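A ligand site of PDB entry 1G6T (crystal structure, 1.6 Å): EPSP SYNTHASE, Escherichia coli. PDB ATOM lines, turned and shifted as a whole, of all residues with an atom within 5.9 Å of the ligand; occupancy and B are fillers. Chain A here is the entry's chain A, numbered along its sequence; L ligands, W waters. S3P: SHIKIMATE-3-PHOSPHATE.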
ATOM      1  N   LYS A  22      -6.995  11.462   8.558  1.00  0.00           N
ATOM      2  CA  LYS A  22      -6.144  12.219   9.477  1.00  0.00           C
ATOM      3  C   LYS A  22      -6.932  12.725  10.675  1.00  0.00           C
ATOM      4  O   LYS A  22      -6.476  12.594  11.810  1.00  0.00           O
ATOM      5  CB  LYS A  22      -5.499  13.392   8.730  1.00  0.00           C
ATOM      6  CG  LYS A  22      -4.677  14.292   9.659  1.00  0.00           C
ATOM      7  CD  LYS A  22      -5.333  15.678   9.822  1.00  0.00           C
ATOM      8  CE  LYS A  22      -5.161  16.509   8.536  1.00  0.00           C
ATOM      9  NZ  LYS A  22      -5.926  17.821   8.621  1.00  0.00           N
ATOM     10  N   SER A  23      -8.123  13.271  10.431  1.00  0.00           N
ATOM     11  CA  SER A  23      -8.951  13.813  11.518  1.00  0.00           C
ATOM     12  C   SER A  23      -9.334  12.744  12.521  1.00  0.00           C
ATOM     13  O   SER A  23      -9.249  12.955  13.712  1.00  0.00           O
ATOM     14  CB  SER A  23     -10.203  14.450  10.939  1.00  0.00           C
ATOM     15  OG  SER A  23      -9.897  15.597  10.134  1.00  0.00           O
ATOM     16  N   VAL A  24      -9.767  11.594  12.009  1.00  0.00           N
ATOM     17  CA  VAL A  24     -10.148  10.512  12.927  1.00  0.00           C
ATOM     18  C   VAL A  24      -8.913   9.921  13.612  1.00  0.00           C
ATOM     19  O   VAL A  24      -8.929   9.639  14.832  1.00  0.00           O
ATOM     20  CB  VAL A  24     -10.890   9.391  12.155  1.00  0.00           C
ATOM     21  CG1 VAL A  24     -11.131   8.187  13.107  1.00  0.00           C
ATOM     22  CG2 VAL A  24     -12.253   9.945  11.618  1.00  0.00           C
ATOM     23  N   ARG A  27      -7.551  12.127  16.588  1.00  0.00           N
ATOM     24  CA  ARG A  27      -8.494  12.131  17.716  1.00  0.00           C
ATOM     25  C   ARG A  27      -8.438  10.763  18.417  1.00  0.00           C
ATOM     26  O   ARG A  27      -8.353  10.724  19.648  1.00  0.00           O
ATOM     27  CB  ARG A  27      -9.920  12.367  17.208  1.00  0.00           C
ATOM     28  CG  ARG A  27     -10.219  13.838  16.835  1.00  0.00           C
ATOM     29  CD  ARG A  27     -11.583  13.907  16.192  1.00  0.00           C
ATOM     30  NE  ARG A  27     -12.061  15.247  15.881  1.00  0.00           N
ATOM     31  CZ  ARG A  27     -11.614  16.033  14.912  1.00  0.00           C
ATOM     32  NH1 ARG A  27     -12.198  17.213  14.728  1.00  0.00           N
ATOM     33  NH2 ARG A  27     -10.552  15.683  14.172  1.00  0.00           N
ATOM     34  N   THR A  97      -4.320  19.170  14.231  1.00  0.00           N
ATOM     35  CA  THR A  97      -5.009  18.156  15.033  1.00  0.00           C
ATOM     36  C   THR A  97      -4.165  17.566  16.179  1.00  0.00           C
ATOM     37  O   THR A  97      -4.642  16.714  16.944  1.00  0.00           O
ATOM     38  CB  THR A  97      -5.600  17.004  14.170  1.00  0.00           C
ATOM     39  OG1 THR A  97      -4.541  16.349  13.458  1.00  0.00           O
ATOM     40  CG2 THR A  97      -6.627  17.570  13.157  1.00  0.00           C
ATOM     41  N   ARG A 100      -3.746  21.803  18.513  1.00  0.00           N
ATOM     42  CA  ARG A 100      -4.880  22.314  19.242  1.00  0.00           C
ATOM     43  C   ARG A 100      -5.345  21.340  20.334  1.00  0.00           C
ATOM     44  O   ARG A 100      -5.462  21.729  21.505  1.00  0.00           O
ATOM     45  CB  ARG A 100      -5.997  22.736  18.274  1.00  0.00           C
ATOM     46  CG  ARG A 100      -5.794  24.146  17.635  1.00  0.00           C
ATOM     47  CD  ARG A 100      -4.606  24.201  16.615  1.00  0.00           C
ATOM     48  NE  ARG A 100      -4.541  25.501  15.925  1.00  0.00           N
ATOM     49  CZ  ARG A 100      -5.119  25.747  14.750  1.00  0.00           C
ATOM     50  NH1 ARG A 100      -5.008  26.934  14.180  1.00  0.00           N
ATOM     51  NH2 ARG A 100      -5.835  24.808  14.123  1.00  0.00           N
ATOM     52  N   ARG A 124       0.023  30.261  12.867  1.00  0.00           N
ATOM     53  CA  ARG A 124      -1.365  29.808  12.830  1.00  0.00           C
ATOM     54  C   ARG A 124      -1.943  30.129  14.196  1.00  0.00           C
ATOM     55  O   ARG A 124      -1.388  29.725  15.243  1.00  0.00           O
ATOM     56  CB  ARG A 124      -1.434  28.319  12.500  1.00  0.00           C
ATOM     57  CG  ARG A 124      -0.991  28.068  11.031  1.00  0.00           C
ATOM     58  CD  ARG A 124      -1.144  26.610  10.640  1.00  0.00           C
ATOM     59  NE  ARG A 124      -2.555  26.217  10.634  1.00  0.00           N
ATOM     60  CZ  ARG A 124      -2.964  24.966  10.537  1.00  0.00           C
ATOM     61  NH1 ARG A 124      -4.268  24.692  10.539  1.00  0.00           N
ATOM     62  NH2 ARG A 124      -2.077  23.983  10.453  1.00  0.00           N
ATOM     63  N   VAL A 168     -13.023  31.257  13.774  1.00  0.00           N
ATOM     64  CA  VAL A 168     -11.773  31.065  13.039  1.00  0.00           C
ATOM     65  C   VAL A 168     -11.415  29.610  12.863  1.00  0.00           C
ATOM     66  O   VAL A 168     -10.979  29.205  11.775  1.00  0.00           O
ATOM     67  CB  VAL A 168     -10.619  31.849  13.696  1.00  0.00           C
ATOM     68  CG1 VAL A 168      -9.258  31.498  13.065  1.00  0.00           C
ATOM     69  CG2 VAL A 168     -10.884  33.350  13.510  1.00  0.00           C
ATOM     70  N   SER A 169     -11.582  28.822  13.916  1.00  0.00           N
ATOM     71  CA  SER A 169     -11.311  27.366  13.793  1.00  0.00           C
ATOM     72  C   SER A 169     -12.215  26.570  14.701  1.00  0.00           C
ATOM     73  O   SER A 169     -12.401  26.919  15.881  1.00  0.00           O
ATOM     74  CB  SER A 169      -9.847  27.009  14.178  1.00  0.00           C
ATOM     75  OG  SER A 169      -9.594  25.590  14.013  1.00  0.00           O
ATOM     76  N   SER A 170     -12.736  25.464  14.171  1.00  0.00           N
ATOM     77  CA  SER A 170     -13.533  24.540  14.975  1.00  0.00           C
ATOM     78  C   SER A 170     -12.574  23.717  15.838  1.00  0.00           C
ATOM     79  O   SER A 170     -13.003  23.097  16.796  1.00  0.00           O
ATOM     80  CB  SER A 170     -14.330  23.550  14.063  1.00  0.00           C
ATOM     81  OG  SER A 170     -13.454  22.693  13.308  1.00  0.00           O
ATOM     82  N   GLN A 171     -11.278  23.732  15.515  1.00  0.00           N
ATOM     83  CA  GLN A 171     -10.355  22.908  16.295  1.00  0.00           C
ATOM     84  C   GLN A 171     -10.210  23.332  17.742  1.00  0.00           C
ATOM     85  O   GLN A 171      -9.859  22.515  18.584  1.00  0.00           O
ATOM     86  CB  GLN A 171      -8.967  22.836  15.642  1.00  0.00           C
ATOM     87  CG  GLN A 171      -9.000  22.120  14.254  1.00  0.00           C
ATOM     88  CD  GLN A 171      -7.596  21.788  13.745  1.00  0.00           C
ATOM     89  OE1 GLN A 171      -6.613  22.141  14.370  1.00  0.00           O
ATOM     90  NE2 GLN A 171      -7.520  21.059  12.632  1.00  0.00           N
ATOM     91  N   THR A 174     -13.117  21.667  19.380  1.00  0.00           N
ATOM     92  CA  THR A 174     -12.827  20.256  19.447  1.00  0.00           C
ATOM     93  C   THR A 174     -11.876  19.951  20.606  1.00  0.00           C
ATOM     94  O   THR A 174     -12.097  19.007  21.381  1.00  0.00           O
ATOM     95  CB  THR A 174     -12.209  19.790  18.111  1.00  0.00           C
ATOM     96  OG1 THR A 174     -13.266  19.451  17.209  1.00  0.00           O
ATOM     97  CG2 THR A 174     -11.306  18.595  18.301  1.00  0.00           C
ATOM     98  N   VAL A 196     -17.481  27.943  12.586  1.00  0.00           N
ATOM     99  CA  VAL A 196     -17.098  27.468  11.259  1.00  0.00           C
ATOM    100  C   VAL A 196     -16.745  25.986  11.337  1.00  0.00           C
ATOM    101  O   VAL A 196     -16.530  25.430  12.421  1.00  0.00           O
ATOM    102  CB  VAL A 196     -15.873  28.201  10.698  1.00  0.00           C
ATOM    103  CG1 VAL A 196     -16.199  29.673  10.495  1.00  0.00           C
ATOM    104  CG2 VAL A 196     -14.696  28.010  11.630  1.00  0.00           C
ATOM    105  N   SER A 197     -16.729  25.354  10.154  1.00  0.00           N
ATOM    106  CA  SER A 197     -16.345  23.942  10.049  1.00  0.00           C
ATOM    107  C   SER A 197     -17.098  23.045  11.005  1.00  0.00           C
ATOM    108  O   SER A 197     -16.535  22.094  11.567  1.00  0.00           O
ATOM    109  CB  SER A 197     -14.830  23.813  10.293  1.00  0.00           C
ATOM    110  OG  SER A 197     -14.116  24.380   9.200  1.00  0.00           O
ATOM    111  N   TYR A 200     -16.768  19.090  11.621  1.00  0.00           N
ATOM    112  CA  TYR A 200     -15.658  18.518  12.391  1.00  0.00           C
ATOM    113  C   TYR A 200     -16.006  18.352  13.838  1.00  0.00           C
ATOM    114  O   TYR A 200     -15.430  17.508  14.529  1.00  0.00           O
ATOM    115  CB  TYR A 200     -14.351  19.348  12.203  1.00  0.00           C
ATOM    116  CG  TYR A 200     -13.794  19.158  10.813  1.00  0.00           C
ATOM    117  CD1 TYR A 200     -14.099  20.060   9.781  1.00  0.00           C
ATOM    118  CD2 TYR A 200     -12.968  18.063  10.522  1.00  0.00           C
ATOM    119  CE1 TYR A 200     -13.597  19.891   8.481  1.00  0.00           C
ATOM    120  CE2 TYR A 200     -12.459  17.880   9.222  1.00  0.00           C
ATOM    121  CZ  TYR A 200     -12.776  18.786   8.226  1.00  0.00           C
ATOM    122  OH  TYR A 200     -12.303  18.618   6.937  1.00  0.00           O
ATOM    123  N   ILE A 203     -17.469  15.006  14.168  1.00  0.00           N
ATOM    124  CA  ILE A 203     -16.455  13.942  14.213  1.00  0.00           C
ATOM    125  C   ILE A 203     -15.952  13.830  15.672  1.00  0.00           C
ATOM    126  O   ILE A 203     -15.810  12.738  16.213  1.00  0.00           O
ATOM    127  CB  ILE A 203     -15.245  14.295  13.277  1.00  0.00           C
ATOM    128  CG1 ILE A 203     -15.717  14.366  11.825  1.00  0.00           C
ATOM    129  CG2 ILE A 203     -14.127  13.278  13.460  1.00  0.00           C
ATOM    130  CD1 ILE A 203     -14.576  14.680  10.823  1.00  0.00           C
ATOM    131  N   THR A 204     -15.630  14.951  16.303  1.00  0.00           N
ATOM    132  CA  THR A 204     -15.139  14.905  17.670  1.00  0.00           C
ATOM    133  C   THR A 204     -16.102  14.230  18.633  1.00  0.00           C
ATOM    134  O   THR A 204     -15.703  13.388  19.441  1.00  0.00           O
ATOM    135  CB  THR A 204     -14.851  16.332  18.147  1.00  0.00           C
ATOM    136  OG1 THR A 204     -13.835  16.875  17.282  1.00  0.00           O
ATOM    137  CG2 THR A 204     -14.354  16.350  19.598  1.00  0.00           C
ATOM    138  N   PRO A 312     -14.285  22.912   3.935  1.00  0.00           N
ATOM    139  CA  PRO A 312     -13.162  23.759   3.553  1.00  0.00           C
ATOM    140  C   PRO A 312     -11.969  23.119   2.898  1.00  0.00           C
ATOM    141  O   PRO A 312     -11.351  23.742   2.012  1.00  0.00           O
ATOM    142  CB  PRO A 312     -12.815  24.481   4.860  1.00  0.00           C
ATOM    143  CG  PRO A 312     -13.199  23.513   5.954  1.00  0.00           C
ATOM    144  CD  PRO A 312     -14.506  22.891   5.390  1.00  0.00           C
ATOM    145  N   ASP A 313     -11.657  21.888   3.294  1.00  0.00           N
ATOM    146  CA  ASP A 313     -10.497  21.216   2.721  1.00  0.00           C
ATOM    147  C   ASP A 313     -10.822  20.638   1.329  1.00  0.00           C
ATOM    148  O   ASP A 313     -10.124  20.947   0.346  1.00  0.00           O
ATOM    149  CB  ASP A 313     -10.044  20.102   3.670  1.00  0.00           C
ATOM    150  CG  ASP A 313      -9.418  20.612   4.965  1.00  0.00           C
ATOM    151  OD1 ASP A 313      -9.123  19.752   5.823  1.00  0.00           O
ATOM    152  OD2 ASP A 313      -9.218  21.843   5.139  1.00  0.00           O
ATOM    153  N   ASN A 336     -11.220  31.043   6.528  1.00  0.00           N
ATOM    154  CA  ASN A 336     -10.141  30.418   7.263  1.00  0.00           C
ATOM    155  C   ASN A 336      -9.147  29.647   6.411  1.00  0.00           C
ATOM    156  O   ASN A 336      -8.174  29.138   6.929  1.00  0.00           O
ATOM    157  CB  ASN A 336     -10.634  29.656   8.503  1.00  0.00           C
ATOM    158  CG  ASN A 336     -11.233  28.332   8.195  1.00  0.00           C
ATOM    159  OD1 ASN A 336     -11.282  27.873   7.052  1.00  0.00           O
ATOM    160  ND2 ASN A 336     -11.683  27.670   9.254  1.00  0.00           N
ATOM    161  N   LYS A 340      -4.537  28.436   7.467  1.00  0.00           N
ATOM    162  CA  LYS A 340      -4.226  27.013   7.475  1.00  0.00           C
ATOM    163  C   LYS A 340      -2.786  26.682   7.049  1.00  0.00           C
ATOM    164  O   LYS A 340      -1.865  27.445   7.395  1.00  0.00           O
ATOM    165  CB  LYS A 340      -5.308  26.279   6.687  1.00  0.00           C
ATOM    166  CG  LYS A 340      -6.615  26.240   7.543  1.00  0.00           C
ATOM    167  CD  LYS A 340      -7.782  25.748   6.747  1.00  0.00           C
ATOM    168  CE  LYS A 340      -8.895  25.518   7.769  1.00  0.00           C
ATOM    169  NZ  LYS A 340     -10.146  25.164   7.142  1.00  0.00           N
ATOM    170  N   GLU A 341      -2.573  25.592   6.330  1.00  0.00           N
ATOM    171  CA  GLU A 341      -1.198  25.183   5.982  1.00  0.00           C
ATOM    172  C   GLU A 341      -0.431  26.318   5.359  1.00  0.00           C
ATOM    173  O   GLU A 341       0.790  26.427   5.531  1.00  0.00           O
ATOM    174  CB  GLU A 341      -1.226  23.936   5.117  1.00  0.00           C
ATOM    175  CG  GLU A 341      -1.414  22.625   5.938  1.00  0.00           C
ATOM    176  CD  GLU A 341      -2.874  22.291   6.370  1.00  0.00           C
ATOM    177  OE1 GLU A 341      -3.780  23.186   6.431  1.00  0.00           O
ATOM    178  OE2 GLU A 341      -3.086  21.089   6.689  1.00  0.00           O
ATOM    179  N   ARG A 344      -4.378  29.792   1.918  1.00  0.00           N
ATOM    180  CA  ARG A 344      -4.852  29.088   0.728  1.00  0.00           C
ATOM    181  C   ARG A 344      -5.618  29.962  -0.276  1.00  0.00           C
ATOM    182  O   ARG A 344      -5.649  29.629  -1.457  1.00  0.00           O
ATOM    183  CB  ARG A 344      -5.649  27.854   1.152  1.00  0.00           C
ATOM    184  CG  ARG A 344      -4.752  26.785   1.797  1.00  0.00           C
ATOM    185  CD  ARG A 344      -5.529  25.730   2.583  1.00  0.00           C
ATOM    186  NE  ARG A 344      -4.730  24.494   2.699  1.00  0.00           N
ATOM    187  CZ  ARG A 344      -5.127  23.415   3.365  1.00  0.00           C
ATOM    188  NH1 ARG A 344      -4.349  22.334   3.389  1.00  0.00           N
ATOM    189  NH2 ARG A 344      -6.293  23.404   4.016  1.00  0.00           N
ATOM    190  N   ARG A 386      -2.230  19.944   0.162  1.00  0.00           N
ATOM    191  CA  ARG A 386      -3.367  20.114  -0.760  1.00  0.00           C
ATOM    192  C   ARG A 386      -3.097  20.952  -1.986  1.00  0.00           C
ATOM    193  O   ARG A 386      -3.753  20.786  -3.014  1.00  0.00           O
ATOM    194  CB  ARG A 386      -4.613  20.612  -0.011  1.00  0.00           C
ATOM    195  CG  ARG A 386      -5.014  19.637   1.112  1.00  0.00           C
ATOM    196  CD  ARG A 386      -6.504  19.819   1.569  1.00  0.00           C
ATOM    197  NE  ARG A 386      -6.660  19.027   2.779  1.00  0.00           N
ATOM    198  CZ  ARG A 386      -6.685  17.689   2.818  1.00  0.00           C
ATOM    199  NH1 ARG A 386      -6.748  17.089   4.007  1.00  0.00           N
ATOM    200  NH2 ARG A 386      -6.758  16.960   1.693  1.00  0.00           N
HETATM  201  C1  S3P L   1     -10.011  19.556  11.061  1.00  0.00           C
HETATM  202  C2  S3P L   1     -10.820  20.701  10.995  1.00  0.00           C
HETATM  203  C3  S3P L   1     -10.674  21.729   9.922  1.00  0.00           C
HETATM  204  C4  S3P L   1      -9.889  21.191   8.720  1.00  0.00           C
HETATM  205  C5  S3P L   1      -8.595  20.512   9.195  1.00  0.00           C
HETATM  206  C6  S3P L   1      -9.002  19.293  10.058  1.00  0.00           C
HETATM  207  C7  S3P L   1     -10.219  18.585  12.189  1.00  0.00           C
HETATM  208  O1  S3P L   1     -10.088  22.982  10.513  1.00  0.00           O
HETATM  209  O2  S3P L   1      -9.644  22.272   7.840  1.00  0.00           O
HETATM  210  O3  S3P L   1      -7.841  20.092   8.071  1.00  0.00           O
HETATM  211  O4  S3P L   1     -10.750  19.040  13.228  1.00  0.00           O
HETATM  212  O5  S3P L   1      -9.866  17.409  12.035  1.00  0.00           O
HETATM  213  P1  S3P L   1     -10.924  24.454  10.899  1.00  0.00           P
HETATM  214  O6  S3P L   1     -11.877  24.126  11.953  1.00  0.00           O
HETATM  215  O7  S3P L   1     -11.572  24.808   9.602  1.00  0.00           O
HETATM  216  O8  S3P L   1      -9.847  25.359  11.393  1.00  0.00           O
HETATM  217  O   HOH W   1     -12.446  20.554  14.781  1.00  0.00           O
HETATM  218  O   HOH W   2      -6.357  22.980   7.721  1.00  0.00           O
HETATM  219  O   HOH W   3      -7.234  24.378  11.447  1.00  0.00           O
HETATM  220  O   HOH W   4      -8.614  27.561  10.896  1.00  0.00           O
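N of Ser 170 lies within hydrogen-bond range of O6 of the ligand (2.7 Å).
OG of Ser 170 is in hydrogen-bond range of O6 of the ligand (2.5 Å).
OD1 of Asp 313 sits at hydrogen-bond distance from O3 of the ligand (2.6 Å).
O7 of the ligand sits at hydrogen-bond distance from OG of Ser 197 (2.6 Å).
An oxygen (O5) of the ligand sits at hydrogen-bond distance from the side-chain hydroxyl of Ser 23 (2.6 Å).
An oxygen (O8) of the ligand is in hydrogen-bond range of the side-chain hydroxyl (OG) of Ser 169.
NH1 of Arg 27 lies within salt-bridge range of O4 of the ligand (2.8 Å).
The side-chain amino group of Lys 340 is in salt-bridge range of an oxygen (O7) of the ligand, at 2.9 Å.
O7 of the ligand is in hydrogen-bond range of ND2 of Asn 336 (2.9 Å).
The side-chain amino group of Lys 22 sits at hydrogen-bond distance from an oxygen (O3) of the ligand (3.0 Å).
The side-chain amino group (NZ) of Lys 340 lies within salt-bridge range of the side-chain carboxylate (OD2) of Asp 313, at 3.99 Å.
The guanidinium group (NH2) of Arg 27 lies within hydrogen-bond range of the backbone carbonyl oxygen (O) of Ser 23.
OG of Ser 169 is in hydrogen-bond range of N of Gln 171, 2.9 Å away.
NH1 of Arg 27 is in hydrogen-bond range of O of Tyr 200 (3.3 Å).
NE of Arg 27 is in hydrogen-bond range of OG1 of Thr 204 (2.8 Å).
O of Val 168 lies within hydrogen-bond range of ND2 of Asn 336, 3.0 Å away.
The backbone carbonyl oxygen (O) of Tyr 200 sits at hydrogen-bond distance from the side-chain hydroxyl (OG1) of Thr 204, at 3.2 Å.
OE1 of Gln 171 lies within hydrogen-bond range of NH2 of Arg 100 (2.8 Å).
Water W4 lies within hydrogen-bond range of O8 of the ligand, O of Val 168 and ND2 of Asn 336.
Water W1 lies within hydrogen-bond range of an oxygen (O4) of the ligand, the side-chain hydroxyl (OG) of Ser 170, the side-chain hydroxyl (OG1) of Thr 174, the guanidinium group (NH1) of Arg 27 and the backbone NH (N) of Gln 171.
Water W3 lies within hydrogen-bond range of O8 of the ligand (2.8 Å), NH2 of Arg 100 (3.1 Å) and NH1 of Arg 124 (3.1 Å).
Water W2 bridges OE1 of Glu 341 and O3 of the ligand.
Thr 97 touches the ligand (CG2 to O5, 3.4 Å).
Gln 171 touches the ligand (NE2 to C1, 3.3 Å).
CD2 of Tyr 200 touches C7 of the ligand, at 3.3 Å.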
